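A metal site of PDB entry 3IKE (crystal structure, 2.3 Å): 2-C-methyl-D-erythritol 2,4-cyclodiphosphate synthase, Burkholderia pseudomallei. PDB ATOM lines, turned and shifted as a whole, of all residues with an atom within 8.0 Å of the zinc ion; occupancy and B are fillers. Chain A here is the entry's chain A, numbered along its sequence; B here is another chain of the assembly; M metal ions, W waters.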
ATOM      1  N   TYR A  13     -33.783 -24.589 -13.654  1.00  0.00           N
ATOM      2  CA  TYR A  13     -33.686 -23.436 -14.525  1.00  0.00           C
ATOM      3  C   TYR A  13     -33.002 -22.297 -13.797  1.00  0.00           C
ATOM      4  O   TYR A  13     -33.260 -22.060 -12.636  1.00  0.00           O
ATOM      5  CB  TYR A  13     -35.117 -22.949 -14.868  1.00  0.00           C
ATOM      6  CG  TYR A  13     -35.157 -21.642 -15.648  1.00  0.00           C
ATOM      7  CD1 TYR A  13     -34.854 -21.613 -17.016  1.00  0.00           C
ATOM      8  CD2 TYR A  13     -35.467 -20.422 -15.022  1.00  0.00           C
ATOM      9  CE1 TYR A  13     -34.874 -20.436 -17.728  1.00  0.00           C
ATOM     10  CE2 TYR A  13     -35.492 -19.235 -15.743  1.00  0.00           C
ATOM     11  CZ  TYR A  13     -35.205 -19.258 -17.103  1.00  0.00           C
ATOM     12  OH  TYR A  13     -35.227 -18.100 -17.860  1.00  0.00           O
ATOM     13  N   ASP A  14     -32.160 -21.562 -14.497  1.00  0.00           N
ATOM     14  CA  ASP A  14     -31.686 -20.303 -13.948  1.00  0.00           C
ATOM     15  C   ASP A  14     -31.351 -19.300 -15.059  1.00  0.00           C
ATOM     16  O   ASP A  14     -30.879 -19.674 -16.136  1.00  0.00           O
ATOM     17  CB  ASP A  14     -30.493 -20.569 -13.018  1.00  0.00           C
ATOM     18  CG  ASP A  14     -30.270 -19.427 -12.006  1.00  0.00           C
ATOM     19  OD1 ASP A  14     -31.206 -18.653 -11.742  1.00  0.00           O
ATOM     20  OD2 ASP A  14     -29.149 -19.274 -11.502  1.00  0.00           O
ATOM     21  N   VAL A  15     -31.583 -18.020 -14.799  1.00  0.00           N
ATOM     22  CA  VAL A  15     -31.062 -16.938 -15.659  1.00  0.00           C
ATOM     23  C   VAL A  15     -30.427 -15.864 -14.777  1.00  0.00           C
ATOM     24  O   VAL A  15     -30.852 -15.640 -13.648  1.00  0.00           O
ATOM     25  CB  VAL A  15     -32.184 -16.332 -16.544  1.00  0.00           C
ATOM     26  CG1 VAL A  15     -33.137 -15.472 -15.718  1.00  0.00           C
ATOM     27  CG2 VAL A  15     -31.587 -15.551 -17.714  1.00  0.00           C
ATOM     28  N   HIS A  16     -29.390 -15.198 -15.301  1.00  0.00           N
ATOM     29  CA  HIS A  16     -28.862 -13.981 -14.680  1.00  0.00           C
ATOM     30  C   HIS A  16     -28.463 -13.026 -15.782  1.00  0.00           C
ATOM     31  O   HIS A  16     -27.990 -13.440 -16.860  1.00  0.00           O
ATOM     32  CB  HIS A  16     -27.634 -14.223 -13.827  1.00  0.00           C
ATOM     33  CG  HIS A  16     -27.903 -14.989 -12.567  1.00  0.00           C
ATOM     34  ND1 HIS A  16     -28.164 -14.372 -11.366  1.00  0.00           N
ATOM     35  CD2 HIS A  16     -27.913 -16.326 -12.323  1.00  0.00           C
ATOM     36  CE1 HIS A  16     -28.367 -15.309 -10.444  1.00  0.00           C
ATOM     37  NE2 HIS A  16     -28.216 -16.493 -11.002  1.00  0.00           N
ATOM     38  N   LEU A  37     -21.917 -12.153 -14.349  1.00  0.00           N
ATOM     39  CA  LEU A  37     -23.312 -12.352 -14.042  1.00  0.00           C
ATOM     40  C   LEU A  37     -23.704 -11.589 -12.800  1.00  0.00           C
ATOM     41  O   LEU A  37     -22.939 -11.514 -11.853  1.00  0.00           O
ATOM     42  CB  LEU A  37     -23.684 -13.843 -13.939  1.00  0.00           C
ATOM     43  CG  LEU A  37     -23.628 -14.611 -15.267  1.00  0.00           C
ATOM     44  CD1 LEU A  37     -23.864 -16.162 -15.069  1.00  0.00           C
ATOM     45  CD2 LEU A  37     -24.599 -13.998 -16.331  1.00  0.00           C
ATOM     46  N   LEU A  38     -24.908 -11.035 -12.800  1.00  0.00           N
ATOM     47  CA  LEU A  38     -25.363 -10.262 -11.648  1.00  0.00           C
ATOM     48  C   LEU A  38     -26.292 -11.053 -10.760  1.00  0.00           C
ATOM     49  O   LEU A  38     -27.322 -11.545 -11.227  1.00  0.00           O
ATOM     50  CB  LEU A  38     -26.049  -8.965 -12.107  1.00  0.00           C
ATOM     51  CG  LEU A  38     -26.700  -8.115 -10.992  1.00  0.00           C
ATOM     52  CD1 LEU A  38     -25.632  -7.298 -10.255  1.00  0.00           C
ATOM     53  CD2 LEU A  38     -27.843  -7.208 -11.529  1.00  0.00           C
ATOM     54  N   GLY A  39     -25.923 -11.155  -9.487  1.00  0.00           N
ATOM     55  CA  GLY A  39     -26.800 -11.689  -8.431  1.00  0.00           C
ATOM     56  C   GLY A  39     -26.313 -11.331  -7.025  1.00  0.00           C
ATOM     57  O   GLY A  39     -25.317 -10.622  -6.847  1.00  0.00           O
ATOM     58  N   HIS A  40     -27.042 -11.830  -6.030  1.00  0.00           N
ATOM     59  CA  HIS A  40     -26.625 -11.744  -4.621  1.00  0.00           C
ATOM     60  C   HIS A  40     -25.348 -12.593  -4.309  1.00  0.00           C
ATOM     61  O   HIS A  40     -24.390 -12.097  -3.663  1.00  0.00           O
ATOM     62  CB  HIS A  40     -27.820 -12.151  -3.751  1.00  0.00           C
ATOM     63  CG  HIS A  40     -27.671 -11.811  -2.291  1.00  0.00           C
ATOM     64  ND1 HIS A  40     -27.787 -10.524  -1.809  1.00  0.00           N
ATOM     65  CD2 HIS A  40     -27.456 -12.612  -1.214  1.00  0.00           C
ATOM     66  CE1 HIS A  40     -27.637 -10.541  -0.491  1.00  0.00           C
ATOM     67  NE2 HIS A  40     -27.444 -11.787  -0.108  1.00  0.00           N
ATOM     68  N   SER A  41     -25.313 -13.852  -4.791  1.00  0.00           N
ATOM     69  CA  SER A  41     -24.134 -14.719  -4.653  1.00  0.00           C
ATOM     70  C   SER A  41     -23.106 -14.371  -5.739  1.00  0.00           C
ATOM     71  O   SER A  41     -23.159 -13.268  -6.330  1.00  0.00           O
ATOM     72  CB  SER A  41     -24.520 -16.217  -4.737  1.00  0.00           C
ATOM     73  OG  SER A  41     -25.278 -16.526  -5.909  1.00  0.00           O
ATOM     74  N   ASP A  42     -22.167 -15.284  -6.006  1.00  0.00           N
ATOM     75  CA  ASP A  42     -21.315 -15.157  -7.213  1.00  0.00           C
ATOM     76  C   ASP A  42     -22.164 -15.306  -8.515  1.00  0.00           C
ATOM     77  O   ASP A  42     -21.631 -15.309  -9.623  1.00  0.00           O
ATOM     78  CB  ASP A  42     -20.187 -16.184  -7.175  1.00  0.00           C
ATOM     79  CG  ASP A  42     -20.690 -17.624  -7.238  1.00  0.00           C
ATOM     80  OD1 ASP A  42     -21.870 -17.851  -7.628  1.00  0.00           O
ATOM     81  OD2 ASP A  42     -19.911 -18.545  -6.897  1.00  0.00           O
ATOM     82  N   ALA A  43     -23.484 -15.459  -8.377  1.00  0.00           N
ATOM     83  CA  ALA A  43     -24.406 -15.563  -9.522  1.00  0.00           C
ATOM     84  C   ALA A  43     -24.077 -16.661 -10.571  1.00  0.00           C
ATOM     85  O   ALA A  43     -24.324 -16.489 -11.786  1.00  0.00           O
ATOM     86  CB  ALA A  43     -24.582 -14.180 -10.212  1.00  0.00           C
ATOM     87  N   ASP A  44     -23.528 -17.781 -10.079  1.00  0.00           N
ATOM     88  CA  ASP A  44     -23.174 -18.914 -10.924  1.00  0.00           C
ATOM     89  C   ASP A  44     -24.434 -19.611 -11.424  1.00  0.00           C
ATOM     90  O   ASP A  44     -24.968 -20.489 -10.739  1.00  0.00           O
ATOM     91  CB  ASP A  44     -22.278 -19.912 -10.179  1.00  0.00           C
ATOM     92  CG  ASP A  44     -21.623 -20.927 -11.114  1.00  0.00           C
ATOM     93  OD1 ASP A  44     -22.277 -21.379 -12.093  1.00  0.00           O
ATOM     94  OD2 ASP A  44     -20.447 -21.286 -10.889  1.00  0.00           O
ATOM     95  N   VAL A  45     -24.864 -19.222 -12.624  1.00  0.00           N
ATOM     96  CA  VAL A  45     -26.152 -19.648 -13.197  1.00  0.00           C
ATOM     97  C   VAL A  45     -26.265 -21.157 -13.368  1.00  0.00           C
ATOM     98  O   VAL A  45     -27.350 -21.755 -13.229  1.00  0.00           O
ATOM     99  CB  VAL A  45     -26.421 -18.911 -14.578  1.00  0.00           C
ATOM    100  CG1 VAL A  45     -25.371 -19.293 -15.650  1.00  0.00           C
ATOM    101  CG2 VAL A  45     -27.886 -19.112 -15.105  1.00  0.00           C
ATOM    102  N   LEU A  46     -25.133 -21.785 -13.684  1.00  0.00           N
ATOM    103  CA  LEU A  46     -25.127 -23.210 -13.944  1.00  0.00           C
ATOM    104  C   LEU A  46     -25.283 -24.003 -12.667  1.00  0.00           C
ATOM    105  O   LEU A  46     -26.097 -24.923 -12.618  1.00  0.00           O
ATOM    106  CB  LEU A  46     -23.889 -23.655 -14.709  1.00  0.00           C
ATOM    107  CG  LEU A  46     -23.725 -25.167 -14.899  1.00  0.00           C
ATOM    108  CD1 LEU A  46     -24.850 -25.772 -15.784  1.00  0.00           C
ATOM    109  CD2 LEU A  46     -22.358 -25.463 -15.529  1.00  0.00           C
ATOM    110  N   LEU A  47     -24.502 -23.670 -11.635  1.00  0.00           N
ATOM    111  CA  LEU A  47     -24.575 -24.411 -10.371  1.00  0.00           C
ATOM    112  C   LEU A  47     -25.917 -24.206  -9.722  1.00  0.00           C
ATOM    113  O   LEU A  47     -26.426 -25.123  -9.075  1.00  0.00           O
ATOM    114  CB  LEU A  47     -23.451 -23.968  -9.418  1.00  0.00           C
ATOM    115  CG  LEU A  47     -22.049 -24.154  -9.998  1.00  0.00           C
ATOM    116  CD1 LEU A  47     -21.046 -23.856  -8.943  1.00  0.00           C
ATOM    117  CD2 LEU A  47     -21.780 -25.625 -10.569  1.00  0.00           C
ATOM    118  N   HIS A  48     -26.503 -23.015  -9.871  1.00  0.00           N
ATOM    119  CA  HIS A  48     -27.833 -22.767  -9.320  1.00  0.00           C
ATOM    120  C   HIS A  48     -28.897 -23.667  -9.933  1.00  0.00           C
ATOM    121  O   HIS A  48     -29.757 -24.212  -9.232  1.00  0.00           O
ATOM    122  CB  HIS A  48     -28.252 -21.312  -9.481  1.00  0.00           C
ATOM    123  CG  HIS A  48     -27.387 -20.360  -8.708  1.00  0.00           C
ATOM    124  ND1 HIS A  48     -27.487 -18.989  -8.820  1.00  0.00           N
ATOM    125  CD2 HIS A  48     -26.398 -20.599  -7.812  1.00  0.00           C
ATOM    126  CE1 HIS A  48     -26.599 -18.417  -8.031  1.00  0.00           C
ATOM    127  NE2 HIS A  48     -25.917 -19.377  -7.416  1.00  0.00           N
ATOM    128  N   ALA A  49     -28.843 -23.785 -11.264  1.00  0.00           N
ATOM    129  CA  ALA A  49     -29.775 -24.639 -11.986  1.00  0.00           C
ATOM    130  C   ALA A  49     -29.596 -26.106 -11.540  1.00  0.00           C
ATOM    131  O   ALA A  49     -30.584 -26.843 -11.320  1.00  0.00           O
ATOM    132  CB  ALA A  49     -29.533 -24.457 -13.536  1.00  0.00           C
ATOM    133  N   ASP A  52     -30.992 -26.539  -8.026  1.00  0.00           N
ATOM    134  CA  ASP A  52     -32.446 -26.678  -8.145  1.00  0.00           C
ATOM    135  C   ASP A  52     -32.874 -28.029  -8.537  1.00  0.00           C
ATOM    136  O   ASP A  52     -33.827 -28.534  -7.978  1.00  0.00           O
ATOM    137  CB  ASP A  52     -33.045 -25.659  -9.116  1.00  0.00           C
ATOM    138  CG  ASP A  52     -33.692 -24.489  -8.380  1.00  0.00           C
ATOM    139  OD1 ASP A  52     -33.578 -24.486  -7.145  1.00  0.00           O
ATOM    140  OD2 ASP A  52     -34.307 -23.578  -9.021  1.00  0.00           O
ATOM    141  N   ILE A  63     -33.753 -23.663  -4.403  1.00  0.00           N
ATOM    142  CA  ILE A  63     -32.579 -22.978  -3.912  1.00  0.00           C
ATOM    143  C   ILE A  63     -32.949 -21.713  -3.148  1.00  0.00           C
ATOM    144  O   ILE A  63     -32.245 -21.339  -2.210  1.00  0.00           O
ATOM    145  CB  ILE A  63     -31.626 -22.630  -5.071  1.00  0.00           C
ATOM    146  CG1 ILE A  63     -30.226 -22.360  -4.552  1.00  0.00           C
ATOM    147  CG2 ILE A  63     -32.215 -21.472  -5.954  1.00  0.00           C
ATOM    148  CD1 ILE A  63     -29.225 -22.062  -5.669  1.00  0.00           C
ATOM    149  N   ASP A  69     -32.480 -15.444  -1.243  1.00  0.00           N
ATOM    150  CA  ASP A  69     -32.021 -14.304  -2.044  1.00  0.00           C
ATOM    151  C   ASP A  69     -31.704 -13.067  -1.187  1.00  0.00           C
ATOM    152  O   ASP A  69     -31.001 -12.140  -1.633  1.00  0.00           O
ATOM    153  CB  ASP A  69     -33.122 -13.945  -3.070  1.00  0.00           C
ATOM    154  CG  ASP A  69     -32.549 -13.441  -4.380  1.00  0.00           C
ATOM    155  OD1 ASP A  69     -31.404 -12.956  -4.381  1.00  0.00           O
ATOM    156  OD2 ASP A  69     -33.251 -13.523  -5.419  1.00  0.00           O
ATOM    157  N   SER A  79     -20.966 -20.326  -4.913  1.00  0.00           N
ATOM    158  CA  SER A  79     -22.013 -21.270  -5.318  1.00  0.00           C
ATOM    159  C   SER A  79     -21.585 -22.761  -5.324  1.00  0.00           C
ATOM    160  O   SER A  79     -22.442 -23.652  -5.249  1.00  0.00           O
ATOM    161  CB  SER A  79     -22.595 -20.862  -6.662  1.00  0.00           C
ATOM    162  OG  SER A  79     -23.412 -19.703  -6.508  1.00  0.00           O
ATOM    163  N   ILE A 152     -27.417 -14.850 -19.363  1.00  0.00           N
ATOM    164  CA  ILE A 152     -27.032 -16.216 -19.642  1.00  0.00           C
ATOM    165  C   ILE A 152     -27.970 -17.135 -18.877  1.00  0.00           C
ATOM    166  O   ILE A 152     -28.281 -16.889 -17.709  1.00  0.00           O
ATOM    167  CB  ILE A 152     -25.556 -16.492 -19.287  1.00  0.00           C
ATOM    168  CG1 ILE A 152     -24.632 -15.670 -20.182  1.00  0.00           C
ATOM    169  CG2 ILE A 152     -25.249 -18.045 -19.329  1.00  0.00           C
ATOM    170  CD1 ILE A 152     -23.120 -15.804 -19.858  1.00  0.00           C
ATOM    171  N   LYS B 138     -39.071 -19.356  -9.652  1.00  0.00           N
ATOM    172  CA  LYS B 138     -37.962 -18.482 -10.076  1.00  0.00           C
ATOM    173  C   LYS B 138     -38.515 -17.190 -10.646  1.00  0.00           C
ATOM    174  O   LYS B 138     -39.625 -17.181 -11.223  1.00  0.00           O
ATOM    175  CB  LYS B 138     -37.127 -19.148 -11.179  1.00  0.00           C
ATOM    176  CG  LYS B 138     -36.328 -20.440 -10.784  1.00  0.00           C
ATOM    177  CD  LYS B 138     -35.045 -20.141  -9.945  1.00  0.00           C
ATOM    178  CE  LYS B 138     -34.125 -19.113 -10.652  1.00  0.00           C
ATOM    179  NZ  LYS B 138     -32.784 -18.839  -9.974  1.00  0.00           N
ATOM    180  N   GLU B 141     -35.317 -12.530 -13.517  1.00  0.00           N
ATOM    181  CA  GLU B 141     -34.298 -11.480 -13.359  1.00  0.00           C
ATOM    182  C   GLU B 141     -34.537 -10.273 -14.292  1.00  0.00           C
ATOM    183  O   GLU B 141     -33.606  -9.690 -14.826  1.00  0.00           O
ATOM    184  CB  GLU B 141     -32.891 -12.096 -13.533  1.00  0.00           C
ATOM    185  CG  GLU B 141     -32.515 -13.083 -12.446  1.00  0.00           C
ATOM    186  CD  GLU B 141     -32.348 -12.420 -11.096  1.00  0.00           C
ATOM    187  OE1 GLU B 141     -31.661 -11.386 -11.038  1.00  0.00           O
ATOM    188  OE2 GLU B 141     -32.925 -12.897 -10.095  1.00  0.00           O
HETATM  189 ZN    ZN M   1     -28.932 -17.976  -9.864  1.00  0.00          ZN
HETATM  190  O   HOH W   1     -32.036 -16.490 -10.477  1.00  0.00           O
HETATM  191  O   HOH W   2     -30.759 -17.612  -8.742  1.00  0.00           O
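NE2 of His 48 lies within hydrogen-bond range of OG of Ser 79 (2.7 Å). The backbone NH (N) of Ile 152 sits at hydrogen-bond distance from the backbone carbonyl oxygen (O) of His 16, 2.9 Å away. ND1 of His 16 sits at hydrogen-bond distance from O of Leu 38. The side-chain hydroxyl (OG) of Ser 41 lies close to a ring nitrogen (NE2) of His 48 (3.3 Å). The side-chain amino group of Lys 138 of chain B lies close to the side-chain carboxylate of Asp 14 (3.97 Å).
Residues that only touch the zinc ion: Lys 138 of chain B. Within 4 Å of the zinc ion: Asp 14, His 16, His 48 and Lys 138 of chain B.
The zinc ion is bound by a ring nitrogen (NE2) of His 16, a ring nitrogen (ND1) of His 48, the side-chain carboxylate (OD2) of Asp 14 and water W2. The zinc ion has four donor atoms within binding distance.
Water W2 lies within hydrogen-bond range of the side-chain amino group of Lys 138 of chain B and the side-chain carboxylate of Asp 14. Water W1 lies within hydrogen-bond range of NZ of Lys 138 of chain B (2.5 Å), OD1 of Asp 14 (2.6 Å) and O of Val 15 (3.5 Å).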
